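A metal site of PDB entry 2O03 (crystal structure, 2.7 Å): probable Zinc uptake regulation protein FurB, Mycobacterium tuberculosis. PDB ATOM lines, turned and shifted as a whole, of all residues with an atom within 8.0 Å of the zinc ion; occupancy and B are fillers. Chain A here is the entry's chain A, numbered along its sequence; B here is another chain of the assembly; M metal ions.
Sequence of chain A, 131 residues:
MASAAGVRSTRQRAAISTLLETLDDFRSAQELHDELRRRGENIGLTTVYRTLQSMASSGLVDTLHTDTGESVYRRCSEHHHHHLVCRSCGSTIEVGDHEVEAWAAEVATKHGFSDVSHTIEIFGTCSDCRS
SG of Cys 86 is bound to the zinc ion, at 2.3 Å.
SG of Cys 89 binds the zinc ion (2.4 Å).
The side-chain sulfur (SG) of Cys 129 is bound to the zinc ion (2.4 Å).
The zinc ion is bound by the side-chain sulfur (SG) of Cys 126, 2.4 Å away.
O of Cys 126 is in hydrogen-bond range of NH1 of Arg 130 (3.5 Å).
The backbone carbonyl oxygen (O) of Cys 89 sits close to the side-chain hydroxyl (OG) of Ser 57, 3.4 Å away.
The side-chain sulfur (SG) of Cys 89 lies close to the backbone NH (N) of Ser 91 (3.6 Å).
The side-chain sulfur (SG) of Cys 86 lies close to the backbone NH (N) of Ser 88.
The backbone carbonyl oxygen of Ser 91 sits at hydrogen-bond distance from the backbone NH of Cys 86 (3.1 Å).
SG of Cys 86 lies close to O of Gly 124 (3.7 Å).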
ATOM      1  N   SER A  57       2.487 -12.824  33.294  1.00  0.00           N
ATOM      2  CA  SER A  57       2.725 -14.258  33.382  1.00  0.00           C
ATOM      3  C   SER A  57       1.626 -15.066  34.079  1.00  0.00           C
ATOM      4  O   SER A  57       1.835 -16.227  34.418  1.00  0.00           O
ATOM      5  CB  SER A  57       4.074 -14.513  34.021  1.00  0.00           C
ATOM      6  OG  SER A  57       4.009 -14.251  35.401  1.00  0.00           O
ATOM      7  N   VAL A  85       3.350 -18.851  24.586  1.00  0.00           N
ATOM      8  CA  VAL A  85       3.652 -18.794  26.019  1.00  0.00           C
ATOM      9  C   VAL A  85       4.972 -19.457  26.423  1.00  0.00           C
ATOM     10  O   VAL A  85       5.326 -20.532  25.918  1.00  0.00           O
ATOM     11  CB  VAL A  85       2.470 -19.306  26.870  1.00  0.00           C
ATOM     12  CG1 VAL A  85       2.666 -18.989  28.367  1.00  0.00           C
ATOM     13  CG2 VAL A  85       1.213 -18.638  26.405  1.00  0.00           C
ATOM     14  N   CYS A  86       5.689 -18.813  27.335  1.00  0.00           N
ATOM     15  CA  CYS A  86       6.893 -19.389  27.917  1.00  0.00           C
ATOM     16  C   CYS A  86       6.583 -20.426  29.002  1.00  0.00           C
ATOM     17  O   CYS A  86       5.962 -20.104  30.006  1.00  0.00           O
ATOM     18  CB  CYS A  86       7.832 -18.317  28.485  1.00  0.00           C
ATOM     19  SG  CYS A  86       9.439 -19.036  28.889  1.00  0.00           S
ATOM     20  N   ARG A  87       7.041 -21.656  28.772  1.00  0.00           N
ATOM     21  CA  ARG A  87       6.890 -22.746  29.757  1.00  0.00           C
ATOM     22  C   ARG A  87       7.470 -22.425  31.130  1.00  0.00           C
ATOM     23  O   ARG A  87       7.002 -22.917  32.138  1.00  0.00           O
ATOM     24  CB  ARG A  87       7.542 -24.046  29.241  1.00  0.00           C
ATOM     25  CG  ARG A  87       6.887 -24.627  27.987  1.00  0.00           C
ATOM     26  CD  ARG A  87       7.223 -26.120  27.770  1.00  0.00           C
ATOM     27  NE  ARG A  87       6.980 -26.499  26.369  1.00  0.00           N
ATOM     28  CZ  ARG A  87       7.824 -26.228  25.362  1.00  0.00           C
ATOM     29  NH1 ARG A  87       8.969 -25.567  25.587  1.00  0.00           N
ATOM     30  NH2 ARG A  87       7.530 -26.617  24.109  1.00  0.00           N
ATOM     31  N   SER A  88       8.491 -21.574  31.167  1.00  0.00           N
ATOM     32  CA  SER A  88       9.246 -21.387  32.395  1.00  0.00           C
ATOM     33  C   SER A  88       8.764 -20.276  33.322  1.00  0.00           C
ATOM     34  O   SER A  88       8.782 -20.435  34.536  1.00  0.00           O
ATOM     35  CB  SER A  88      10.716 -21.195  32.063  1.00  0.00           C
ATOM     36  OG  SER A  88      11.318 -22.457  31.957  1.00  0.00           O
ATOM     37  N   CYS A  89       8.351 -19.143  32.741  1.00  0.00           N
ATOM     38  CA  CYS A  89       7.884 -17.992  33.508  1.00  0.00           C
ATOM     39  C   CYS A  89       6.429 -17.569  33.200  1.00  0.00           C
ATOM     40  O   CYS A  89       5.867 -16.737  33.932  1.00  0.00           O
ATOM     41  CB  CYS A  89       8.804 -16.800  33.259  1.00  0.00           C
ATOM     42  SG  CYS A  89       8.815 -16.253  31.560  1.00  0.00           S
ATOM     43  N   GLY A  90       5.845 -18.095  32.127  1.00  0.00           N
ATOM     44  CA  GLY A  90       4.459 -17.804  31.767  1.00  0.00           C
ATOM     45  C   GLY A  90       4.251 -16.569  30.887  1.00  0.00           C
ATOM     46  O   GLY A  90       3.095 -16.218  30.545  1.00  0.00           O
ATOM     47  N   SER A  91       5.347 -15.891  30.536  1.00  0.00           N
ATOM     48  CA  SER A  91       5.317 -14.741  29.633  1.00  0.00           C
ATOM     49  C   SER A  91       4.398 -14.992  28.410  1.00  0.00           C
ATOM     50  O   SER A  91       4.641 -15.902  27.608  1.00  0.00           O
ATOM     51  CB  SER A  91       6.759 -14.429  29.195  1.00  0.00           C
ATOM     52  OG  SER A  91       6.852 -13.210  28.475  1.00  0.00           O
ATOM     53  N   THR A  92       3.335 -14.179  28.285  1.00  0.00           N
ATOM     54  CA  THR A  92       2.345 -14.343  27.220  1.00  0.00           C
ATOM     55  C   THR A  92       2.520 -13.284  26.111  1.00  0.00           C
ATOM     56  O   THR A  92       2.478 -12.072  26.388  1.00  0.00           O
ATOM     57  CB  THR A  92       0.887 -14.224  27.751  1.00  0.00           C
ATOM     58  OG1 THR A  92       0.783 -14.787  29.061  1.00  0.00           O
ATOM     59  CG2 THR A  92      -0.070 -14.907  26.820  1.00  0.00           C
ATOM     60  N   GLY A 124       7.167 -22.493  24.196  1.00  0.00           N
ATOM     61  CA  GLY A 124       8.627 -22.563  24.029  1.00  0.00           C
ATOM     62  C   GLY A 124       9.316 -21.970  25.249  1.00  0.00           C
ATOM     63  O   GLY A 124       8.655 -21.408  26.114  1.00  0.00           O
ATOM     64  N   THR A 125      10.633 -22.099  25.329  1.00  0.00           N
ATOM     65  CA  THR A 125      11.416 -21.537  26.434  1.00  0.00           C
ATOM     66  C   THR A 125      11.982 -20.183  25.994  1.00  0.00           C
ATOM     67  O   THR A 125      12.724 -20.089  25.016  1.00  0.00           O
ATOM     68  CB  THR A 125      12.507 -22.511  26.900  1.00  0.00           C
ATOM     69  N   CYS A 126      11.601 -19.116  26.700  1.00  0.00           N
ATOM     70  CA  CYS A 126      11.839 -17.747  26.209  1.00  0.00           C
ATOM     71  C   CYS A 126      13.302 -17.271  26.280  1.00  0.00           C
ATOM     72  O   CYS A 126      14.160 -17.918  26.899  1.00  0.00           O
ATOM     73  CB  CYS A 126      10.880 -16.735  26.878  1.00  0.00           C
ATOM     74  SG  CYS A 126      11.474 -16.059  28.421  1.00  0.00           S
ATOM     75  N   SER A 127      13.565 -16.129  25.656  1.00  0.00           N
ATOM     76  CA  SER A 127      14.917 -15.595  25.473  1.00  0.00           C
ATOM     77  C   SER A 127      15.587 -15.232  26.815  1.00  0.00           C
ATOM     78  O   SER A 127      16.723 -15.633  27.100  1.00  0.00           O
ATOM     79  CB  SER A 127      14.845 -14.372  24.551  1.00  0.00           C
ATOM     80  OG  SER A 127      16.123 -13.820  24.349  1.00  0.00           O
ATOM     81  N   ASP A 128      14.851 -14.469  27.609  1.00  0.00           N
ATOM     82  CA  ASP A 128      15.096 -14.246  29.026  1.00  0.00           C
ATOM     83  C   ASP A 128      15.303 -15.550  29.830  1.00  0.00           C
ATOM     84  O   ASP A 128      16.135 -15.611  30.727  1.00  0.00           O
ATOM     85  CB  ASP A 128      13.878 -13.509  29.567  1.00  0.00           C
ATOM     86  CG  ASP A 128      14.222 -12.532  30.663  1.00  0.00           C
ATOM     87  OD1 ASP A 128      15.081 -11.662  30.442  1.00  0.00           O
ATOM     88  OD2 ASP A 128      13.594 -12.630  31.746  1.00  0.00           O
ATOM     89  N   CYS A 129      14.529 -16.591  29.503  1.00  0.00           N
ATOM     90  CA  CYS A 129      14.565 -17.843  30.272  1.00  0.00           C
ATOM     91  C   CYS A 129      15.737 -18.798  30.006  1.00  0.00           C
ATOM     92  O   CYS A 129      15.966 -19.723  30.798  1.00  0.00           O
ATOM     93  CB  CYS A 129      13.250 -18.596  30.149  1.00  0.00           C
ATOM     94  SG  CYS A 129      12.172 -18.216  31.495  1.00  0.00           S
ATOM     95  N   ARG A 130      16.450 -18.602  28.890  1.00  0.00           N
ATOM     96  CA  ARG A 130      17.765 -19.221  28.748  1.00  0.00           C
ATOM     97  C   ARG A 130      18.759 -18.316  29.473  1.00  0.00           C
ATOM     98  O   ARG A 130      19.942 -18.626  29.549  1.00  0.00           O
ATOM     99  CB  ARG A 130      18.155 -19.354  27.280  1.00  0.00           C
ATOM    100  CG  ARG A 130      17.524 -20.522  26.553  1.00  0.00           C
ATOM    101  CD  ARG A 130      17.930 -20.555  25.067  1.00  0.00           C
ATOM    102  NE  ARG A 130      17.667 -19.293  24.356  1.00  0.00           N
ATOM    103  CZ  ARG A 130      16.472 -18.886  23.926  1.00  0.00           C
ATOM    104  NH1 ARG A 130      15.370 -19.623  24.119  1.00  0.00           N
ATOM    105  NH2 ARG A 130      16.366 -17.730  23.289  1.00  0.00           N
ATOM    106  N   PHE B 113      12.422 -17.777  20.819  1.00  0.00           N
ATOM    107  CA  PHE B 113      12.016 -18.883  21.688  1.00  0.00           C
ATOM    108  C   PHE B 113      12.721 -20.205  21.294  1.00  0.00           C
ATOM    109  O   PHE B 113      12.790 -20.530  20.108  1.00  0.00           O
ATOM    110  CB  PHE B 113      10.479 -19.092  21.598  1.00  0.00           C
ATOM    111  CG  PHE B 113       9.656 -18.335  22.643  1.00  0.00           C
ATOM    112  CD1 PHE B 113       9.967 -17.019  23.016  1.00  0.00           C
ATOM    113  CD2 PHE B 113       8.517 -18.940  23.216  1.00  0.00           C
ATOM    114  CE1 PHE B 113       9.174 -16.332  23.969  1.00  0.00           C
ATOM    115  CE2 PHE B 113       7.713 -18.248  24.161  1.00  0.00           C
ATOM    116  CZ  PHE B 113       8.056 -16.947  24.535  1.00  0.00           C
HETATM  117 ZN    ZN M   1      10.408 -17.333  30.149  1.00  0.00          ZN
